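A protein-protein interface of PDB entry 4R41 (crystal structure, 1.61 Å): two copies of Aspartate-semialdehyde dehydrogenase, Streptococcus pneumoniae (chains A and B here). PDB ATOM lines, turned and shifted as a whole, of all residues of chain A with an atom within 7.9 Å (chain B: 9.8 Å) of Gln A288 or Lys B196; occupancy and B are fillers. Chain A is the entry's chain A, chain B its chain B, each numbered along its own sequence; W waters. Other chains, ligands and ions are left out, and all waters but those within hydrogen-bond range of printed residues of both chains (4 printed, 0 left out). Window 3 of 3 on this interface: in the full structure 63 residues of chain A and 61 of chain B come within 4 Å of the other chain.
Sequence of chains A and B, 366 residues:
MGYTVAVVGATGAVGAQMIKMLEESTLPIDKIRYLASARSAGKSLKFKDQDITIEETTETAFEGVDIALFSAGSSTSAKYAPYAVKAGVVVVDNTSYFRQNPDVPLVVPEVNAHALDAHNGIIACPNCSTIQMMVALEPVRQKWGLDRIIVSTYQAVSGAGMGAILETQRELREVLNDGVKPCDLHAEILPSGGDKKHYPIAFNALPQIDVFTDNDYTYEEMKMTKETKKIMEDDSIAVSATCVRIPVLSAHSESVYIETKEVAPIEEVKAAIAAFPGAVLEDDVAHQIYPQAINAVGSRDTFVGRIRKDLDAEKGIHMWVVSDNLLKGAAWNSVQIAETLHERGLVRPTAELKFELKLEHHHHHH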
ATOM      1  N   GLU A 282       9.775  22.668  -9.716  1.00  0.00           N
ATOM      2  CA  GLU A 282      10.874  22.037 -10.428  1.00  0.00           C
ATOM      3  C   GLU A 282      11.607  21.184  -9.421  1.00  0.00           C
ATOM      4  O   GLU A 282      12.531  21.640  -8.747  1.00  0.00           O
ATOM      5  CB  GLU A 282      11.806  23.067 -11.066  1.00  0.00           C
ATOM      6  CG  GLU A 282      11.282  23.623 -12.374  1.00  0.00           C
ATOM      7  CD  GLU A 282      12.335  24.410 -13.126  1.00  0.00           C
ATOM      8  OE1 GLU A 282      13.136  25.106 -12.481  1.00  0.00           O
ATOM      9  OE2 GLU A 282      12.352  24.350 -14.367  1.00  0.00           O
ATOM     10  N   ASP A 283      11.183  19.923  -9.317  1.00  0.00           N
ATOM     11  CA  ASP A 283      11.566  19.126  -8.138  1.00  0.00           C
ATOM     12  C   ASP A 283      11.438  17.652  -8.441  1.00  0.00           C
ATOM     13  O   ASP A 283      10.373  17.073  -8.306  1.00  0.00           O
ATOM     14  CB  ASP A 283      10.682  19.510  -6.934  1.00  0.00           C
ATOM     15  CG  ASP A 283      11.300  19.104  -5.575  1.00  0.00           C
ATOM     16  OD1 ASP A 283      12.140  18.183  -5.551  1.00  0.00           O
ATOM     17  OD2 ASP A 283      10.927  19.717  -4.548  1.00  0.00           O
ATOM     18  N   ASP A 284      12.534  17.055  -8.871  1.00  0.00           N
ATOM     19  CA  ASP A 284      12.556  15.605  -9.154  1.00  0.00           C
ATOM     20  C   ASP A 284      13.991  15.197  -8.914  1.00  0.00           C
ATOM     21  O   ASP A 284      14.788  15.138  -9.848  1.00  0.00           O
ATOM     22  CB  ASP A 284      12.135  15.342 -10.615  1.00  0.00           C
ATOM     23  CG  ASP A 284      12.198  13.876 -10.997  1.00  0.00           C
ATOM     24  OD1 ASP A 284      12.513  13.022 -10.124  1.00  0.00           O
ATOM     25  OD2 ASP A 284      11.938  13.587 -12.190  1.00  0.00           O
ATOM     26  N   VAL A 285      14.326  14.948  -7.657  1.00  0.00           N
ATOM     27  CA  VAL A 285      15.727  14.706  -7.310  1.00  0.00           C
ATOM     28  C   VAL A 285      16.261  13.412  -7.912  1.00  0.00           C
ATOM     29  O   VAL A 285      17.454  13.315  -8.192  1.00  0.00           O
ATOM     30  CB  VAL A 285      15.979  14.785  -5.794  1.00  0.00           C
ATOM     31  CG1 VAL A 285      15.547  16.149  -5.288  1.00  0.00           C
ATOM     32  CG2 VAL A 285      15.246  13.673  -5.051  1.00  0.00           C
ATOM     33  N   ALA A 286      15.364  12.444  -8.158  1.00  0.00           N
ATOM     34  CA  ALA A 286      15.741  11.208  -8.870  1.00  0.00           C
ATOM     35  C   ALA A 286      16.407  11.515 -10.207  1.00  0.00           C
ATOM     36  O   ALA A 286      17.249  10.739 -10.680  1.00  0.00           O
ATOM     37  CB  ALA A 286      14.520  10.305  -9.089  1.00  0.00           C
ATOM     38  N   HIS A 287      16.023  12.634 -10.831  1.00  0.00           N
ATOM     39  CA  HIS A 287      16.633  13.046 -12.087  1.00  0.00           C
ATOM     40  C   HIS A 287      17.363  14.397 -11.967  1.00  0.00           C
ATOM     41  O   HIS A 287      17.564  15.100 -12.971  1.00  0.00           O
ATOM     42  CB  HIS A 287      15.587  13.079 -13.206  1.00  0.00           C
ATOM     43  CG  HIS A 287      14.795  11.808 -13.319  1.00  0.00           C
ATOM     44  ND1 HIS A 287      15.280  10.685 -13.957  1.00  0.00           N
ATOM     45  CD2 HIS A 287      13.572  11.472 -12.844  1.00  0.00           C
ATOM     46  CE1 HIS A 287      14.377   9.721 -13.894  1.00  0.00           C
ATOM     47  NE2 HIS A 287      13.333  10.171 -13.222  1.00  0.00           N
ATOM     48  N   GLN A 288      17.782  14.733 -10.739  1.00  0.00           N
ATOM     49  CA  GLN A 288      18.585  15.925 -10.490  1.00  0.00           C
ATOM     50  C   GLN A 288      17.902  17.178 -11.037  1.00  0.00           C
ATOM     51  O   GLN A 288      18.563  18.034 -11.629  1.00  0.00           O
ATOM     52  CB  GLN A 288      19.959  15.790 -11.138  1.00  0.00           C
ATOM     53  CG  GLN A 288      20.826  14.722 -10.478  1.00  0.00           C
ATOM     54  CD  GLN A 288      22.098  14.539 -11.240  1.00  0.00           C
ATOM     55  OE1 GLN A 288      22.187  13.668 -12.113  1.00  0.00           O
ATOM     56  NE2 GLN A 288      23.093  15.386 -10.956  1.00  0.00           N
ATOM     57  N   ILE A 289      16.591  17.260 -10.838  1.00  0.00           N
ATOM     58  CA  ILE A 289      15.817  18.422 -11.290  1.00  0.00           C
ATOM     59  C   ILE A 289      15.563  19.317 -10.091  1.00  0.00           C
ATOM     60  O   ILE A 289      15.014  18.882  -9.071  1.00  0.00           O
ATOM     61  CB  ILE A 289      14.457  18.037 -11.946  1.00  0.00           C
ATOM     62  CG1 ILE A 289      14.653  17.177 -13.208  1.00  0.00           C
ATOM     63  CG2 ILE A 289      13.647  19.297 -12.253  1.00  0.00           C
ATOM     64  CD1 ILE A 289      15.618  17.730 -14.233  1.00  0.00           C
ATOM     65  N   TYR A 290      16.022  20.559 -10.216  1.00  0.00           N
ATOM     66  CA  TYR A 290      15.832  21.600  -9.197  1.00  0.00           C
ATOM     67  C   TYR A 290      16.053  22.952  -9.892  1.00  0.00           C
ATOM     68  O   TYR A 290      16.689  23.008 -10.969  1.00  0.00           O
ATOM     69  CB  TYR A 290      16.809  21.403  -8.013  1.00  0.00           C
ATOM     70  CG  TYR A 290      18.163  20.845  -8.400  1.00  0.00           C
ATOM     71  CD1 TYR A 290      19.079  21.613  -9.127  1.00  0.00           C
ATOM     72  CD2 TYR A 290      18.522  19.536  -8.054  1.00  0.00           C
ATOM     73  CE1 TYR A 290      20.310  21.104  -9.497  1.00  0.00           C
ATOM     74  CE2 TYR A 290      19.763  19.008  -8.413  1.00  0.00           C
ATOM     75  CZ  TYR A 290      20.645  19.789  -9.125  1.00  0.00           C
ATOM     76  OH  TYR A 290      21.870  19.293  -9.482  1.00  0.00           O
ATOM     77  N   PRO A 291      15.552  24.043  -9.289  1.00  0.00           N
ATOM     78  CA  PRO A 291      15.748  25.344  -9.910  1.00  0.00           C
ATOM     79  C   PRO A 291      17.234  25.746  -9.976  1.00  0.00           C
ATOM     80  O   PRO A 291      18.002  25.453  -9.061  1.00  0.00           O
ATOM     81  CB  PRO A 291      14.988  26.291  -8.975  1.00  0.00           C
ATOM     82  CG  PRO A 291      13.933  25.433  -8.338  1.00  0.00           C
ATOM     83  CD  PRO A 291      14.657  24.123  -8.112  1.00  0.00           C
ATOM     84  N   GLN A 292      17.619  26.376 -11.079  1.00  0.00           N
ATOM     85  CA  GLN A 292      18.991  26.872 -11.268  1.00  0.00           C
ATOM     86  C   GLN A 292      18.941  28.270 -11.857  1.00  0.00           C
ATOM     87  O   GLN A 292      18.211  28.511 -12.817  1.00  0.00           O
ATOM     88  CB  GLN A 292      19.759  26.007 -12.247  1.00  0.00           C
ATOM     89  CG  GLN A 292      19.950  24.572 -11.793  1.00  0.00           C
ATOM     90  CD  GLN A 292      20.759  23.806 -12.799  1.00  0.00           C
ATOM     91  OE1 GLN A 292      21.728  24.317 -13.343  1.00  0.00           O
ATOM     92  NE2 GLN A 292      20.356  22.577 -13.061  1.00  0.00           N
ATOM     93  N   ARG A 306      13.902  21.388  -4.336  1.00  0.00           N
ATOM     94  CA  ARG A 306      14.537  20.833  -3.147  1.00  0.00           C
ATOM     95  C   ARG A 306      13.579  20.854  -1.959  1.00  0.00           C
ATOM     96  O   ARG A 306      14.007  21.013  -0.806  1.00  0.00           O
ATOM     97  CB  ARG A 306      15.847  21.595  -2.780  1.00  0.00           C
ATOM     98  CG  ARG A 306      16.994  21.579  -3.811  1.00  0.00           C
ATOM     99  CD  ARG A 306      17.596  20.192  -4.070  1.00  0.00           C
ATOM    100  NE  ARG A 306      17.625  19.381  -2.858  1.00  0.00           N
ATOM    101  CZ  ARG A 306      18.567  19.416  -1.913  1.00  0.00           C
ATOM    102  NH1 ARG A 306      19.661  20.182  -2.033  1.00  0.00           N
ATOM    103  NH2 ARG A 306      18.423  18.632  -0.832  1.00  0.00           N
ATOM    104  N   HIS B 186      28.701  23.399 -21.897  1.00  0.00           N
ATOM    105  CA  HIS B 186      28.868  21.960 -21.694  1.00  0.00           C
ATOM    106  C   HIS B 186      29.651  21.722 -20.404  1.00  0.00           C
ATOM    107  O   HIS B 186      30.633  22.406 -20.132  1.00  0.00           O
ATOM    108  CB  HIS B 186      29.568  21.281 -22.880  1.00  0.00           C
ATOM    109  CG  HIS B 186      29.565  19.784 -22.790  1.00  0.00           C
ATOM    110  ND1 HIS B 186      30.696  19.051 -22.488  1.00  0.00           N
ATOM    111  CD2 HIS B 186      28.557  18.885 -22.911  1.00  0.00           C
ATOM    112  CE1 HIS B 186      30.390  17.765 -22.447  1.00  0.00           C
ATOM    113  NE2 HIS B 186      29.097  17.638 -22.694  1.00  0.00           N
ATOM    114  N   ALA B 187      29.163  20.778 -19.609  1.00  0.00           N
ATOM    115  CA  ALA B 187      29.751  20.410 -18.331  1.00  0.00           C
ATOM    116  C   ALA B 187      29.882  18.900 -18.277  1.00  0.00           C
ATOM    117  O   ALA B 187      29.012  18.181 -18.793  1.00  0.00           O
ATOM    118  CB  ALA B 187      28.848  20.879 -17.201  1.00  0.00           C
ATOM    119  N   GLU B 188      30.934  18.428 -17.605  1.00  0.00           N
ATOM    120  CA  GLU B 188      31.206  16.997 -17.471  1.00  0.00           C
ATOM    121  C   GLU B 188      31.365  16.506 -16.029  1.00  0.00           C
ATOM    122  O   GLU B 188      31.328  15.308 -15.779  1.00  0.00           O
ATOM    123  CB  GLU B 188      32.447  16.611 -18.291  1.00  0.00           C
ATOM    124  CG  GLU B 188      32.161  16.503 -19.782  1.00  0.00           C
ATOM    125  CD  GLU B 188      33.399  16.298 -20.644  1.00  0.00           C
ATOM    126  OE1 GLU B 188      34.498  16.007 -20.113  1.00  0.00           O
ATOM    127  OE2 GLU B 188      33.267  16.425 -21.881  1.00  0.00           O
ATOM    128  N   ILE B 189      31.556  17.421 -15.084  1.00  0.00           N
ATOM    129  CA  ILE B 189      31.853  17.018 -13.707  1.00  0.00           C
ATOM    130  C   ILE B 189      30.785  17.490 -12.722  1.00  0.00           C
ATOM    131  O   ILE B 189      30.103  16.675 -12.111  1.00  0.00           O
ATOM    132  CB  ILE B 189      33.261  17.479 -13.262  1.00  0.00           C
ATOM    133  CG1 ILE B 189      34.339  16.766 -14.107  1.00  0.00           C
ATOM    134  CG2 ILE B 189      33.486  17.191 -11.783  1.00  0.00           C
ATOM    135  CD1 ILE B 189      35.622  17.547 -14.286  1.00  0.00           C
ATOM    136  N   LEU B 190      30.641  18.801 -12.561  1.00  0.00           N
ATOM    137  CA  LEU B 190      29.691  19.297 -11.570  1.00  0.00           C
ATOM    138  C   LEU B 190      28.229  19.043 -12.002  1.00  0.00           C
ATOM    139  O   LEU B 190      27.961  18.955 -13.193  1.00  0.00           O
ATOM    140  CB  LEU B 190      29.954  20.783 -11.293  1.00  0.00           C
ATOM    141  CG  LEU B 190      31.317  21.015 -10.631  1.00  0.00           C
ATOM    142  CD1 LEU B 190      31.752  22.456 -10.853  1.00  0.00           C
ATOM    143  CD2 LEU B 190      31.288  20.654  -9.143  1.00  0.00           C
ATOM    144  N   PRO B 191      27.278  18.937 -11.042  1.00  0.00           N
ATOM    145  CA  PRO B 191      27.459  19.075  -9.585  1.00  0.00           C
ATOM    146  C   PRO B 191      28.221  17.913  -8.930  1.00  0.00           C
ATOM    147  O   PRO B 191      28.939  18.135  -7.960  1.00  0.00           O
ATOM    148  CB  PRO B 191      26.018  19.124  -9.058  1.00  0.00           C
ATOM    149  CG  PRO B 191      25.182  18.455 -10.115  1.00  0.00           C
ATOM    150  CD  PRO B 191      25.847  18.868 -11.405  1.00  0.00           C
ATOM    151  N   SER B 192      28.073  16.702  -9.467  1.00  0.00           N
ATOM    152  CA  SER B 192      28.713  15.513  -8.887  1.00  0.00           C
ATOM    153  C   SER B 192      29.275  14.575  -9.955  1.00  0.00           C
ATOM    154  O   SER B 192      28.533  14.053 -10.804  1.00  0.00           O
ATOM    155  CB  SER B 192      27.737  14.748  -7.988  1.00  0.00           C
ATOM    156  OG  SER B 192      28.345  13.535  -7.543  1.00  0.00           O
ATOM    157  N   GLY B 193      30.585  14.350  -9.881  1.00  0.00           N
ATOM    158  CA  GLY B 193      31.294  13.481 -10.834  1.00  0.00           C
ATOM    159  C   GLY B 193      30.637  12.121 -10.937  1.00  0.00           C
ATOM    160  O   GLY B 193      30.630  11.512 -12.001  1.00  0.00           O
ATOM    161  N   GLY B 194      30.056  11.663  -9.834  1.00  0.00           N
ATOM    162  CA  GLY B 194      29.450  10.339  -9.778  1.00  0.00           C
ATOM    163  C   GLY B 194      27.945  10.283  -9.997  1.00  0.00           C
ATOM    164  O   GLY B 194      27.325   9.232  -9.768  1.00  0.00           O
ATOM    165  N   ASP B 195      27.343  11.389 -10.432  1.00  0.00           N
ATOM    166  CA  ASP B 195      25.910  11.372 -10.757  1.00  0.00           C
ATOM    167  C   ASP B 195      25.715  11.411 -12.273  1.00  0.00           C
ATOM    168  O   ASP B 195      26.668  11.631 -13.009  1.00  0.00           O
ATOM    169  CB  ASP B 195      25.137  12.503 -10.043  1.00  0.00           C
ATOM    170  CG  ASP B 195      23.745  12.051  -9.564  1.00  0.00           C
ATOM    171  OD1 ASP B 195      23.252  11.008 -10.057  1.00  0.00           O
ATOM    172  OD2 ASP B 195      23.134  12.730  -8.697  1.00  0.00           O
ATOM    173  N   LYS B 196      24.484  11.205 -12.730  1.00  0.00           N
ATOM    174  CA  LYS B 196      24.194  11.002 -14.152  1.00  0.00           C
ATOM    175  C   LYS B 196      24.271  12.255 -15.021  1.00  0.00           C
ATOM    176  O   LYS B 196      24.770  12.189 -16.149  1.00  0.00           O
ATOM    177  CB  LYS B 196      22.819  10.347 -14.326  1.00  0.00           C
ATOM    178  CG  LYS B 196      22.674   9.004 -13.625  1.00  0.00           C
ATOM    179  CD  LYS B 196      21.311   8.388 -13.882  1.00  0.00           C
ATOM    180  CE  LYS B 196      21.005   7.333 -12.836  1.00  0.00           C
ATOM    181  NZ  LYS B 196      19.537   7.115 -12.748  1.00  0.00           N
ATOM    182  N   LYS B 197      23.774  13.384 -14.501  1.00  0.00           N
ATOM    183  CA  LYS B 197      23.647  14.621 -15.283  1.00  0.00           C
ATOM    184  C   LYS B 197      24.609  15.676 -14.760  1.00  0.00           C
ATOM    185  O   LYS B 197      24.844  15.759 -13.552  1.00  0.00           O
ATOM    186  CB  LYS B 197      22.215  15.169 -15.241  1.00  0.00           C
ATOM    187  CG  LYS B 197      21.180  14.200 -15.807  1.00  0.00           C
ATOM    188  CD  LYS B 197      20.042  14.948 -16.458  1.00  0.00           C
ATOM    189  CE  LYS B 197      18.831  14.958 -15.564  1.00  0.00           C
ATOM    190  NZ  LYS B 197      17.870  15.977 -16.032  1.00  0.00           N
ATOM    191  N   HIS B 198      25.161  16.469 -15.673  1.00  0.00           N
ATOM    192  CA  HIS B 198      26.138  17.485 -15.301  1.00  0.00           C
ATOM    193  C   HIS B 198      25.680  18.852 -15.766  1.00  0.00           C
ATOM    194  O   HIS B 198      25.083  18.981 -16.835  1.00  0.00           O
ATOM    195  CB  HIS B 198      27.530  17.121 -15.826  1.00  0.00           C
ATOM    196  CG  HIS B 198      27.950  15.752 -15.405  1.00  0.00           C
ATOM    197  ND1 HIS B 198      28.459  15.487 -14.154  1.00  0.00           N
ATOM    198  CD2 HIS B 198      27.828  14.554 -16.028  1.00  0.00           C
ATOM    199  CE1 HIS B 198      28.684  14.189 -14.039  1.00  0.00           C
ATOM    200  NE2 HIS B 198      28.300  13.601 -15.159  1.00  0.00           N
ATOM    201  N   TYR B 199      25.910  19.854 -14.918  1.00  0.00           N
ATOM    202  CA  TYR B 199      25.403  21.208 -15.164  1.00  0.00           C
ATOM    203  C   TYR B 199      26.507  22.250 -15.001  1.00  0.00           C
ATOM    204  O   TYR B 199      27.444  22.059 -14.207  1.00  0.00           O
ATOM    205  CB  TYR B 199      24.269  21.552 -14.182  1.00  0.00           C
ATOM    206  CG  TYR B 199      23.090  20.620 -14.174  1.00  0.00           C
ATOM    207  CD1 TYR B 199      22.353  20.362 -15.338  1.00  0.00           C
ATOM    208  CD2 TYR B 199      22.683  20.011 -12.981  1.00  0.00           C
ATOM    209  CE1 TYR B 199      21.256  19.503 -15.307  1.00  0.00           C
ATOM    210  CE2 TYR B 199      21.573  19.171 -12.939  1.00  0.00           C
ATOM    211  CZ  TYR B 199      20.874  18.903 -14.110  1.00  0.00           C
ATOM    212  OH  TYR B 199      19.780  18.069 -14.036  1.00  0.00           O
ATOM    213  N   LEU B 206      24.425  25.787  -7.700  1.00  0.00           N
ATOM    214  CA  LEU B 206      23.895  24.421  -7.856  1.00  0.00           C
ATOM    215  C   LEU B 206      23.547  23.840  -6.486  1.00  0.00           C
ATOM    216  O   LEU B 206      24.445  23.576  -5.700  1.00  0.00           O
ATOM    217  CB  LEU B 206      24.910  23.519  -8.599  1.00  0.00           C
ATOM    218  CG  LEU B 206      25.140  23.804 -10.091  1.00  0.00           C
ATOM    219  CD1 LEU B 206      26.306  23.004 -10.678  1.00  0.00           C
ATOM    220  CD2 LEU B 206      23.847  23.451 -10.847  1.00  0.00           C
ATOM    221  N   PRO B 207      22.249  23.633  -6.196  1.00  0.00           N
ATOM    222  CA  PRO B 207      21.818  23.118  -4.885  1.00  0.00           C
ATOM    223  C   PRO B 207      21.977  21.577  -4.789  1.00  0.00           C
ATOM    224  O   PRO B 207      21.081  20.868  -4.332  1.00  0.00           O
ATOM    225  CB  PRO B 207      20.341  23.538  -4.836  1.00  0.00           C
ATOM    226  CG  PRO B 207      19.911  23.429  -6.272  1.00  0.00           C
ATOM    227  CD  PRO B 207      21.093  23.892  -7.084  1.00  0.00           C
ATOM    228  N   GLN B 208      23.116  21.087  -5.251  1.00  0.00           N
ATOM    229  CA  GLN B 208      23.473  19.665  -5.149  1.00  0.00           C
ATOM    230  C   GLN B 208      24.956  19.509  -4.943  1.00  0.00           C
ATOM    231  O   GLN B 208      25.760  19.948  -5.763  1.00  0.00           O
ATOM    232  CB  GLN B 208      23.039  18.866  -6.392  1.00  0.00           C
ATOM    233  CG  GLN B 208      23.326  17.374  -6.223  1.00  0.00           C
ATOM    234  CD  GLN B 208      23.142  16.553  -7.490  1.00  0.00           C
ATOM    235  OE1 GLN B 208      22.544  17.009  -8.474  1.00  0.00           O
ATOM    236  NE2 GLN B 208      23.634  15.310  -7.456  1.00  0.00           N
ATOM    237  N   ILE B 209      25.320  18.871  -3.831  1.00  0.00           N
ATOM    238  CA  ILE B 209      26.683  18.411  -3.621  1.00  0.00           C
ATOM    239  C   ILE B 209      26.601  16.941  -3.198  1.00  0.00           C
ATOM    240  O   ILE B 209      25.792  16.583  -2.334  1.00  0.00           O
ATOM    241  CB  ILE B 209      27.428  19.284  -2.586  1.00  0.00           C
ATOM    242  CG1 ILE B 209      27.529  20.724  -3.134  1.00  0.00           C
ATOM    243  CG2 ILE B 209      28.823  18.714  -2.280  1.00  0.00           C
ATOM    244  CD1 ILE B 209      28.227  21.718  -2.241  1.00  0.00           C
ATOM    245  N   ASP B 210      27.421  16.115  -3.840  1.00  0.00           N
ATOM    246  CA  ASP B 210      27.326  14.646  -3.771  1.00  0.00           C
ATOM    247  C   ASP B 210      25.985  14.207  -4.396  1.00  0.00           C
ATOM    248  O   ASP B 210      25.316  14.997  -5.084  1.00  0.00           O
ATOM    249  CB  ASP B 210      27.495  14.161  -2.326  1.00  0.00           C
ATOM    250  CG  ASP B 210      28.140  12.780  -2.238  1.00  0.00           C
ATOM    251  OD1 ASP B 210      27.726  11.863  -2.983  1.00  0.00           O
ATOM    252  OD2 ASP B 210      29.067  12.636  -1.410  1.00  0.00           O
ATOM    253  N   VAL B 211      25.594  12.964  -4.181  1.00  0.00           N
ATOM    254  CA  VAL B 211      24.350  12.454  -4.752  1.00  0.00           C
ATOM    255  C   VAL B 211      23.212  12.473  -3.743  1.00  0.00           C
ATOM    256  O   VAL B 211      23.421  12.679  -2.542  1.00  0.00           O
ATOM    257  CB  VAL B 211      24.551  11.047  -5.380  1.00  0.00           C
ATOM    258  CG1 VAL B 211      25.674  11.094  -6.417  1.00  0.00           C
ATOM    259  CG2 VAL B 211      24.900  10.022  -4.322  1.00  0.00           C
ATOM    260  N   PHE B 212      22.000  12.243  -4.224  1.00  0.00           N
ATOM    261  CA  PHE B 212      20.854  12.248  -3.350  1.00  0.00           C
ATOM    262  C   PHE B 212      20.705  10.947  -2.559  1.00  0.00           C
ATOM    263  O   PHE B 212      21.000   9.864  -3.071  1.00  0.00           O
ATOM    264  CB  PHE B 212      19.599  12.588  -4.151  1.00  0.00           C
ATOM    265  CG  PHE B 212      19.500  14.056  -4.496  1.00  0.00           C
ATOM    266  CD1 PHE B 212      18.983  14.962  -3.571  1.00  0.00           C
ATOM    267  CD2 PHE B 212      19.975  14.532  -5.717  1.00  0.00           C
ATOM    268  CE1 PHE B 212      18.908  16.319  -3.873  1.00  0.00           C
ATOM    269  CE2 PHE B 212      19.896  15.895  -6.033  1.00  0.00           C
ATOM    270  CZ  PHE B 212      19.366  16.779  -5.103  1.00  0.00           C
ATOM    271  N   ASP B 216      15.766  12.661   0.348  1.00  0.00           N
ATOM    272  CA  ASP B 216      15.811  13.852  -0.541  1.00  0.00           C
ATOM    273  C   ASP B 216      16.810  14.930  -0.106  1.00  0.00           C
ATOM    274  O   ASP B 216      16.909  15.987  -0.736  1.00  0.00           O
ATOM    275  CB  ASP B 216      14.409  14.439  -0.768  1.00  0.00           C
ATOM    276  CG  ASP B 216      13.469  13.438  -1.442  1.00  0.00           C
ATOM    277  OD1 ASP B 216      13.947  12.537  -2.159  1.00  0.00           O
ATOM    278  OD2 ASP B 216      12.253  13.555  -1.241  1.00  0.00           O
ATOM    279  N   THR B 218      20.931  15.498   0.138  1.00  0.00           N
ATOM    280  CA  THR B 218      22.079  14.900  -0.512  1.00  0.00           C
ATOM    281  C   THR B 218      22.972  14.240   0.541  1.00  0.00           C
ATOM    282  O   THR B 218      22.847  14.519   1.741  1.00  0.00           O
ATOM    283  CB  THR B 218      22.938  15.934  -1.273  1.00  0.00           C
ATOM    284  OG1 THR B 218      23.481  16.877  -0.332  1.00  0.00           O
ATOM    285  CG2 THR B 218      22.093  16.662  -2.346  1.00  0.00           C
HETATM  286  O   HOH W   1      18.090  20.745 -12.560  1.00  0.00           O
HETATM  287  O   HOH W   2      20.560  10.510 -10.267  1.00  0.00           O
HETATM  288  O   HOH W   3      15.407  17.701  -2.203  1.00  0.00           O
HETATM  289  O   HOH W   4      26.425  15.645 -11.435  1.00  0.00           O
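The backbone carbonyl oxygen (O) of His A287 sits close to the side-chain amino group (NZ) of Lys B197 (3.2 Å).
NE2 of Gln A288 lies close to OD2 of Asp B195, at 3.5 Å.
N of Lys B196 sits at hydrogen-bond distance from OE1 of Gln A288 (3.4 Å).
The backbone NH of Lys B197 is in hydrogen-bond range of the side-chain amide oxygen of Gln A288 (2.9 Å).
The backbone carbonyl oxygen of Gln A288 is in hydrogen-bond range of the side-chain hydroxyl of Tyr B199, at 2.7 Å.
NE2 of Gln A288 is in hydrogen-bond range of OE1 of Gln B208, at 3.0 Å.
The side-chain hydroxyl (OH) of Tyr A290 is in hydrogen-bond range of the side-chain amide oxygen (OE1) of Gln B208.
The guanidinium group (NH1) of Arg A306 sits at hydrogen-bond distance from the backbone carbonyl oxygen (O) of Pro B207 (2.8 Å).
O of Asp B216 sits at hydrogen-bond distance from NH2 of Arg A306.
The side-chain carboxylate (OD2) of Asp A283 lies within hydrogen-bond range of the backbone NH (N) of Arg A306.
O of Leu B190 sits at hydrogen-bond distance from N of Tyr B199 (2.8 Å).
O of Asp B195 lies within hydrogen-bond range of NE2 of His B198, at 3.3 Å.
OD2 of Asp B195 is in hydrogen-bond range of NE2 of Gln B208 (2.9 Å).
The side-chain amide nitrogen (NE2) of Gln B208 is in hydrogen-bond range of the backbone carbonyl oxygen (O) of Asp B210 (2.9 Å).
Phe B212 touches Val A285.
Asp B216 touches Val A285 (OD1 to CG2, 3.4 Å).
Tyr B199 touches His A287.
Ile A289 touches Lys B197 (CD1 to NZ, 3.4 Å).
Tyr A290 touches Pro B191.
Tyr A290 touches Tyr B199.
Tyr A290 touches Pro B207 (CD1 to CG, 3.5 Å).
Tyr A290 touches Phe B212.
Gln A292 touches Tyr B199.
Leu B206 touches Gln A292 (CD2 to OE1, 3.4 Å).
Asp A284 touches none of the printed residues of chain B.
Ala A286 touches none of the printed residues of chain B.
Ile A289 touches just one residue of chain B: Lys B197 (3.4 Å).
Of the printed residues of chain B, Arg A306 touches Pro B207 (2.8 Å), Phe B212 (3.5 Å) and Asp B216 (3.0 Å).
Of the printed residues of chain A, Asp B195 touches Gln A288 (3.3 Å).
Lys B196 touches just one residue of chain A: Gln A288.
Of the printed residues of chain A, Leu B206 touches Gln A292.
Ile B209 touches none of the printed residues of chain A.
The nearest residue of chain B that does not touch Gln A288 is Phe B212 (4.6 Å).
The nearest residue of chain A that does not touch Lys B196 is Ala A286 (4.8 Å).
The nearest printed residue of chain B that does not touch Tyr A290 is Leu B206 (4.5 Å).
Hydrophobic or aromatic side chains of chain A that line the printed part of chain B: Val A285, Ile A289 and Tyr A290.
Printed residues of chain B that touch a printed residue of chain A: Pro B191, Asp B195, Lys B196, Lys B197, Tyr B199, Leu B206, Pro B207, Gln B208, Phe B212 and Asp B216.
Hydrophobic or aromatic side chains of chain B that line the printed part of chain A: Pro B191, Tyr B199, Leu B206, Pro B207 and Phe B212.
Along chain B the printed residues that touch a printed residue of chain A span positions 191 to 216.
Among the printed residues, no Asp or Glu carboxylate lies within 4 Å of a Lys or Arg side-chain nitrogen of the other chain.
No position is printed for both chains.
Of the 22 pairs that touch across the chains among the printed residues, none has its exchanged pair printed and touching as well.
Water W4 lies within hydrogen-bond range of O of Lys B197 (2.6 Å), O of Ser B192 (2.7 Å), NE2 of Gln A288 (3.4 Å) and ND1 of His B198 (3.4 Å).
Water W3 bridges the backbone carbonyl oxygen of Asp B216 (2.7 Å) and the guanidinium group of Arg A306 (2.9 Å).
Water W2 bridges OD1 of Asp B195 and O of Ala A286.
Water W1 lies within hydrogen-bond range of O of Gln A288 (2.9 Å), NE2 of Gln A292 (3.0 Å), O of Tyr A290 (3.1 Å) and OH of Tyr B199 (3.5 Å).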
